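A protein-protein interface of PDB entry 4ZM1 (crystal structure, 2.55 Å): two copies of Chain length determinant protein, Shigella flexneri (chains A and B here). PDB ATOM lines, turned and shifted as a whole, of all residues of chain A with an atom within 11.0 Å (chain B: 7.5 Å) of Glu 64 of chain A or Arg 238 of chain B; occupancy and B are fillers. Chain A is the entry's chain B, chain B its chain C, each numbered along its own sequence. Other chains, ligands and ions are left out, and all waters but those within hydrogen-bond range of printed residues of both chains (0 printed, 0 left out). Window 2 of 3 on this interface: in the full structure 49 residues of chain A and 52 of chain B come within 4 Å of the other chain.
O of Leu 235 of chain B is in hydrogen-bond range of ND2 of Asn 62 of chain A, 2.9 Å away.
The side-chain amide oxygen of Asn 62 of chain A is in hydrogen-bond range of the backbone NH of Ile 237 of chain B.
The backbone carbonyl oxygen (O) of Gln 63 of chain A is in hydrogen-bond range of the guanidinium group (NH2) of Arg 238 of chain B (3.5 Å).
O of Glu 64 of chain A is in hydrogen-bond range of NH2 of Arg 238 of chain B.
O of Leu 60 of chain A lies close to OE1 of Gln 63 of chain A (3.0 Å).
The side-chain carboxylate (OE1) of Glu 67 of chain A lies close to the side-chain amide oxygen (OE1) of Gln 63 of chain A (2.9 Å).
Among the printed residues, merely in contact across the chains: Asn 62 of chain A with Pro 236 of chain B (3.3 Å) and Gln 63 of chain A with Ile 237 of chain B (3.98 Å).
Glu 64 of chain A touches one residue of chain B.
Of the printed residues of chain A, Arg 238 of chain B touches Gln 63 and Glu 64.
No residue of chain A comes within 4 Å of Trp 6 of chain B.
Of the printed residues of chain B, Gln 63 of chain A touches Ile 237 (3.98 Å) and Arg 238 (3.5 Å).
Printed residues of chain B within 4 Å of Asn 62 of chain A: Leu 235 (2.9 Å), Pro 236 (3.3 Å) and Ile 237 (3.1 Å).
Of the printed residues of chain A, Leu 235 of chain B touches Asn 62.
The nearest residue of chain B that does not touch Glu 64 of chain A is Ile 237 of chain B (4.3 Å).
Of the 11 printed residues of chain A, 3 touch a printed residue of chain B.
Of the 10 printed residues of chain B, 4 touch a printed residue of chain A.
Printed residues of chain B that touch a printed residue of chain A: Leu 235, Pro 236, Ile 237 and Arg 238.
Hydrophobic or aromatic side chains of chain B within 4 Å of the printed part of chain A: Ile 237.
Along chain B the printed residues that touch a printed residue of chain A span positions 235 to 238.
Among the printed residues, no Asp or Glu carboxylate lies within 4 Å of a Lys or Arg side-chain nitrogen of the other chain.
No position is printed for both chains.
Of the 6 pairs that touch across the chains among the printed residues, none has its exchanged pair printed and touching as well.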
ATOM      1  N   GLU A  58      20.881  25.813  11.463  1.00  0.00           N
ATOM      2  CA  GLU A  58      20.030  26.674  12.289  1.00  0.00           C
ATOM      3  C   GLU A  58      18.563  26.603  11.866  1.00  0.00           C
ATOM      4  O   GLU A  58      17.684  26.721  12.715  1.00  0.00           O
ATOM      5  CB  GLU A  58      20.507  28.134  12.235  1.00  0.00           C
ATOM      6  CG  GLU A  58      21.610  28.481  13.225  1.00  0.00           C
ATOM      7  CD  GLU A  58      21.221  28.568  14.689  1.00  0.00           C
ATOM      8  OE1 GLU A  58      20.008  28.635  15.005  1.00  0.00           O
ATOM      9  OE2 GLU A  58      22.148  28.595  15.528  1.00  0.00           O
ATOM     10  N   THR A  59      18.294  26.421  10.566  1.00  0.00           N
ATOM     11  CA  THR A  59      16.922  26.343  10.066  1.00  0.00           C
ATOM     12  C   THR A  59      16.335  24.961  10.381  1.00  0.00           C
ATOM     13  O   THR A  59      15.176  24.881  10.794  1.00  0.00           O
ATOM     14  CB  THR A  59      16.822  26.706   8.576  1.00  0.00           C
ATOM     15  OG1 THR A  59      17.692  25.892   7.808  1.00  0.00           O
ATOM     16  CG2 THR A  59      17.078  28.180   8.305  1.00  0.00           C
ATOM     17  N   LEU A  60      17.151  23.893  10.251  1.00  0.00           N
ATOM     18  CA  LEU A  60      16.731  22.514  10.527  1.00  0.00           C
ATOM     19  C   LEU A  60      16.394  22.292  12.024  1.00  0.00           C
ATOM     20  O   LEU A  60      15.597  21.412  12.347  1.00  0.00           O
ATOM     21  CB  LEU A  60      17.788  21.501  10.049  1.00  0.00           C
ATOM     22  CG  LEU A  60      17.824  21.180   8.538  1.00  0.00           C
ATOM     23  CD1 LEU A  60      19.005  20.279   8.213  1.00  0.00           C
ATOM     24  CD2 LEU A  60      16.513  20.518   8.047  1.00  0.00           C
ATOM     25  N   ASP A  61      16.963  23.115  12.916  1.00  0.00           N
ATOM     26  CA  ASP A  61      16.721  23.109  14.356  1.00  0.00           C
ATOM     27  C   ASP A  61      15.442  23.893  14.693  1.00  0.00           C
ATOM     28  O   ASP A  61      14.744  23.560  15.652  1.00  0.00           O
ATOM     29  CB  ASP A  61      17.926  23.718  15.091  1.00  0.00           C
ATOM     30  CG  ASP A  61      17.946  23.487  16.590  1.00  0.00           C
ATOM     31  OD1 ASP A  61      18.052  22.306  17.010  1.00  0.00           O
ATOM     32  OD2 ASP A  61      17.927  24.486  17.344  1.00  0.00           O
ATOM     33  N   ASN A  62      15.136  24.930  13.909  1.00  0.00           N
ATOM     34  CA  ASN A  62      13.961  25.779  14.125  1.00  0.00           C
ATOM     35  C   ASN A  62      12.710  25.219  13.397  1.00  0.00           C
ATOM     36  O   ASN A  62      12.103  25.896  12.560  1.00  0.00           O
ATOM     37  CB  ASN A  62      14.258  27.223  13.708  1.00  0.00           C
ATOM     38  CG  ASN A  62      13.318  28.231  14.297  1.00  0.00           C
ATOM     39  OD1 ASN A  62      13.045  28.235  15.492  1.00  0.00           O
ATOM     40  ND2 ASN A  62      12.842  29.139  13.474  1.00  0.00           N
ATOM     41  N   GLN A  63      12.326  23.983  13.753  1.00  0.00           N
ATOM     42  CA  GLN A  63      11.174  23.270  13.199  1.00  0.00           C
ATOM     43  C   GLN A  63      10.297  22.669  14.314  1.00  0.00           C
ATOM     44  O   GLN A  63      10.770  22.535  15.449  1.00  0.00           O
ATOM     45  CB  GLN A  63      11.657  22.136  12.282  1.00  0.00           C
ATOM     46  CG  GLN A  63      12.293  22.587  10.975  1.00  0.00           C
ATOM     47  CD  GLN A  63      12.603  21.396  10.105  1.00  0.00           C
ATOM     48  OE1 GLN A  63      13.436  20.550  10.440  1.00  0.00           O
ATOM     49  NE2 GLN A  63      11.913  21.288   8.979  1.00  0.00           N
ATOM     50  N   GLU A  64       9.039  22.257  13.983  1.00  0.00           N
ATOM     51  CA  GLU A  64       8.153  21.565  14.935  1.00  0.00           C
ATOM     52  C   GLU A  64       8.858  20.286  15.391  1.00  0.00           C
ATOM     53  O   GLU A  64       8.877  19.994  16.585  1.00  0.00           O
ATOM     54  CB  GLU A  64       6.766  21.263  14.330  1.00  0.00           C
ATOM     55  CG  GLU A  64       5.774  22.412  14.429  1.00  0.00           C
ATOM     56  CD  GLU A  64       4.356  22.090  13.988  1.00  0.00           C
ATOM     57  OE1 GLU A  64       3.909  22.659  12.966  1.00  0.00           O
ATOM     58  OE2 GLU A  64       3.683  21.291  14.678  1.00  0.00           O
ATOM     59  N   GLU A  65       9.496  19.565  14.436  1.00  0.00           N
ATOM     60  CA  GLU A  65      10.322  18.375  14.663  1.00  0.00           C
ATOM     61  C   GLU A  65      11.760  18.747  14.288  1.00  0.00           C
ATOM     62  O   GLU A  65      12.150  18.673  13.111  1.00  0.00           O
ATOM     63  CB  GLU A  65       9.813  17.162  13.871  1.00  0.00           C
ATOM     64  CG  GLU A  65       8.657  16.440  14.540  1.00  0.00           C
ATOM     65  CD  GLU A  65       7.885  15.475  13.656  1.00  0.00           C
ATOM     66  OE1 GLU A  65       7.597  15.834  12.489  1.00  0.00           O
ATOM     67  OE2 GLU A  65       7.519  14.382  14.150  1.00  0.00           O
ATOM     68  N   PRO A  66      12.544  19.257  15.266  1.00  0.00           N
ATOM     69  CA  PRO A  66      13.899  19.733  14.952  1.00  0.00           C
ATOM     70  C   PRO A  66      14.868  18.629  14.568  1.00  0.00           C
ATOM     71  O   PRO A  66      14.854  17.547  15.150  1.00  0.00           O
ATOM     72  CB  PRO A  66      14.349  20.392  16.262  1.00  0.00           C
ATOM     73  CG  PRO A  66      13.112  20.629  17.036  1.00  0.00           C
ATOM     74  CD  PRO A  66      12.227  19.480  16.688  1.00  0.00           C
ATOM     75  N   GLU A  67      15.743  18.933  13.611  1.00  0.00           N
ATOM     76  CA  GLU A  67      16.766  18.003  13.147  1.00  0.00           C
ATOM     77  C   GLU A  67      18.138  18.478  13.613  1.00  0.00           C
ATOM     78  O   GLU A  67      18.396  19.672  13.623  1.00  0.00           O
ATOM     79  CB  GLU A  67      16.708  17.870  11.617  1.00  0.00           C
ATOM     80  CG  GLU A  67      15.507  17.077  11.144  1.00  0.00           C
ATOM     81  CD  GLU A  67      15.245  17.180   9.658  1.00  0.00           C
ATOM     82  OE1 GLU A  67      14.517  18.113   9.253  1.00  0.00           O
ATOM     83  OE2 GLU A  67      15.752  16.325   8.898  1.00  0.00           O
ATOM     84  N   LYS A  68      19.005  17.554  14.026  1.00  0.00           N
ATOM     85  CA  LYS A  68      20.338  17.949  14.452  1.00  0.00           C
ATOM     86  C   LYS A  68      21.336  17.721  13.315  1.00  0.00           C
ATOM     87  O   LYS A  68      21.656  16.589  12.947  1.00  0.00           O
ATOM     88  CB  LYS A  68      20.782  17.253  15.753  1.00  0.00           C
ATOM     89  CG  LYS A  68      21.791  18.099  16.549  1.00  0.00           C
ATOM     90  CD  LYS A  68      21.960  17.638  18.000  1.00  0.00           C
ATOM     91  CE  LYS A  68      20.864  18.150  18.929  1.00  0.00           C
ATOM     92  NZ  LYS A  68      20.829  17.441  20.246  1.00  0.00           N
ATOM     93  N   LYS B   5      10.317  34.569  26.478  1.00  0.00           N
ATOM     94  CA  LYS B   5      11.655  34.892  25.974  1.00  0.00           C
ATOM     95  C   LYS B   5      11.988  34.047  24.735  1.00  0.00           C
ATOM     96  O   LYS B   5      12.272  32.857  24.856  1.00  0.00           O
ATOM     97  CB  LYS B   5      12.728  34.704  27.067  1.00  0.00           C
ATOM     98  CG  LYS B   5      12.560  35.619  28.288  1.00  0.00           C
ATOM     99  CD  LYS B   5      13.781  36.514  28.547  1.00  0.00           C
ATOM    100  CE  LYS B   5      14.900  35.838  29.316  1.00  0.00           C
ATOM    101  NZ  LYS B   5      15.803  35.051  28.430  1.00  0.00           N
ATOM    102  N   TRP B   6      11.912  34.659  23.551  1.00  0.00           N
ATOM    103  CA  TRP B   6      12.185  33.996  22.278  1.00  0.00           C
ATOM    104  C   TRP B   6      13.450  34.586  21.656  1.00  0.00           C
ATOM    105  O   TRP B   6      13.557  35.813  21.540  1.00  0.00           O
ATOM    106  CB  TRP B   6      11.003  34.152  21.293  1.00  0.00           C
ATOM    107  CG  TRP B   6       9.648  33.759  21.810  1.00  0.00           C
ATOM    108  CD1 TRP B   6       8.910  34.414  22.752  1.00  0.00           C
ATOM    109  CD2 TRP B   6       8.808  32.713  21.300  1.00  0.00           C
ATOM    110  NE1 TRP B   6       7.696  33.790  22.924  1.00  0.00           N
ATOM    111  CE2 TRP B   6       7.599  32.750  22.035  1.00  0.00           C
ATOM    112  CE3 TRP B   6       8.976  31.714  20.326  1.00  0.00           C
ATOM    113  CZ2 TRP B   6       6.581  31.805  21.851  1.00  0.00           C
ATOM    114  CZ3 TRP B   6       7.949  30.802  20.121  1.00  0.00           C
ATOM    115  CH2 TRP B   6       6.773  30.847  20.882  1.00  0.00           C
ATOM    116  N   THR B   7      14.408  33.727  21.255  1.00  0.00           N
ATOM    117  CA  THR B   7      15.633  34.207  20.609  1.00  0.00           C
ATOM    118  C   THR B   7      15.532  34.058  19.094  1.00  0.00           C
ATOM    119  O   THR B   7      15.316  32.957  18.590  1.00  0.00           O
ATOM    120  CB  THR B   7      16.915  33.495  21.133  1.00  0.00           C
ATOM    121  OG1 THR B   7      17.013  33.583  22.556  1.00  0.00           O
ATOM    122  CG2 THR B   7      18.180  34.059  20.521  1.00  0.00           C
ATOM    123  N   ALA B  91       8.186  35.954  19.287  1.00  0.00           N
ATOM    124  CA  ALA B  91       8.961  35.451  18.147  1.00  0.00           C
ATOM    125  C   ALA B  91       9.013  36.497  17.016  1.00  0.00           C
ATOM    126  O   ALA B  91      10.059  36.692  16.384  1.00  0.00           O
ATOM    127  CB  ALA B  91       8.342  34.165  17.632  1.00  0.00           C
ATOM    128  N   LEU B 235      12.294  33.235  12.663  1.00  0.00           N
ATOM    129  CA  LEU B 235      11.037  33.364  13.421  1.00  0.00           C
ATOM    130  C   LEU B 235      11.031  32.152  14.342  1.00  0.00           C
ATOM    131  O   LEU B 235      10.746  31.061  13.850  1.00  0.00           O
ATOM    132  CB  LEU B 235       9.787  33.450  12.503  1.00  0.00           C
ATOM    133  CG  LEU B 235       8.413  33.539  13.213  1.00  0.00           C
ATOM    134  CD1 LEU B 235       8.147  34.931  13.759  1.00  0.00           C
ATOM    135  CD2 LEU B 235       7.282  33.139  12.287  1.00  0.00           C
ATOM    136  N   PRO B 236      11.497  32.277  15.620  1.00  0.00           N
ATOM    137  CA  PRO B 236      11.633  31.082  16.481  1.00  0.00           C
ATOM    138  C   PRO B 236      10.306  30.392  16.765  1.00  0.00           C
ATOM    139  O   PRO B 236       9.340  31.063  17.115  1.00  0.00           O
ATOM    140  CB  PRO B 236      12.277  31.625  17.762  1.00  0.00           C
ATOM    141  CG  PRO B 236      11.997  33.080  17.759  1.00  0.00           C
ATOM    142  CD  PRO B 236      11.934  33.501  16.327  1.00  0.00           C
ATOM    143  N   ILE B 237      10.256  29.055  16.594  1.00  0.00           N
ATOM    144  CA  ILE B 237       9.037  28.252  16.804  1.00  0.00           C
ATOM    145  C   ILE B 237       8.912  27.862  18.308  1.00  0.00           C
ATOM    146  O   ILE B 237       7.801  27.587  18.771  1.00  0.00           O
ATOM    147  CB  ILE B 237       8.986  27.035  15.816  1.00  0.00           C
ATOM    148  CG1 ILE B 237       8.888  27.549  14.342  1.00  0.00           C
ATOM    149  CG2 ILE B 237       7.829  26.077  16.119  1.00  0.00           C
ATOM    150  CD1 ILE B 237       8.827  26.482  13.173  1.00  0.00           C
ATOM    151  N   ARG B 238      10.018  27.915  19.077  1.00  0.00           N
ATOM    152  CA  ARG B 238       9.975  27.602  20.511  1.00  0.00           C
ATOM    153  C   ARG B 238      10.795  28.611  21.337  1.00  0.00           C
ATOM    154  O   ARG B 238      11.694  29.269  20.798  1.00  0.00           O
ATOM    155  CB  ARG B 238      10.411  26.149  20.803  1.00  0.00           C
ATOM    156  CG  ARG B 238      11.682  25.662  20.109  1.00  0.00           C
ATOM    157  CD  ARG B 238      11.845  24.156  20.225  1.00  0.00           C
ATOM    158  NE  ARG B 238      11.042  23.417  19.245  1.00  0.00           N
ATOM    159  CZ  ARG B 238       9.879  22.822  19.509  1.00  0.00           C
ATOM    160  NH1 ARG B 238       9.354  22.881  20.728  1.00  0.00           N
ATOM    161  NH2 ARG B 238       9.230  22.168  18.554  1.00  0.00           N
ATOM    162  N   ARG B 239      10.436  28.761  22.632  1.00  0.00           N
ATOM    163  CA  ARG B 239      11.097  29.669  23.575  1.00  0.00           C
ATOM    164  C   ARG B 239      12.421  29.081  24.071  1.00  0.00           C
ATOM    165  O   ARG B 239      12.519  27.879  24.291  1.00  0.00           O
ATOM    166  CB  ARG B 239      10.182  29.991  24.767  1.00  0.00           C
ATOM    167  CG  ARG B 239       9.084  30.998  24.444  1.00  0.00           C
ATOM    168  CD  ARG B 239       8.024  31.134  25.539  1.00  0.00           C
ATOM    169  NE  ARG B 239       7.214  29.920  25.699  1.00  0.00           N
ATOM    170  CZ  ARG B 239       5.883  29.886  25.727  1.00  0.00           C
ATOM    171  NH1 ARG B 239       5.178  31.008  25.606  1.00  0.00           N
ATOM    172  NH2 ARG B 239       5.246  28.732  25.876  1.00  0.00           N
ATOM    173  N   ASP B 240      13.428  29.950  24.244  1.00  0.00           N
ATOM    174  CA  ASP B 240      14.811  29.695  24.688  1.00  0.00           C
ATOM    175  C   ASP B 240      15.650  30.951  24.436  1.00  0.00           C
ATOM    176  O   ASP B 240      15.386  31.684  23.478  1.00  0.00           O
ATOM    177  CB  ASP B 240      15.446  28.475  23.975  1.00  0.00           C
ATOM    178  CG  ASP B 240      16.600  27.827  24.718  1.00  0.00           C
ATOM    179  OD1 ASP B 240      17.754  27.955  24.249  1.00  0.00           O
ATOM    180  OD2 ASP B 240      16.346  27.156  25.743  1.00  0.00           O
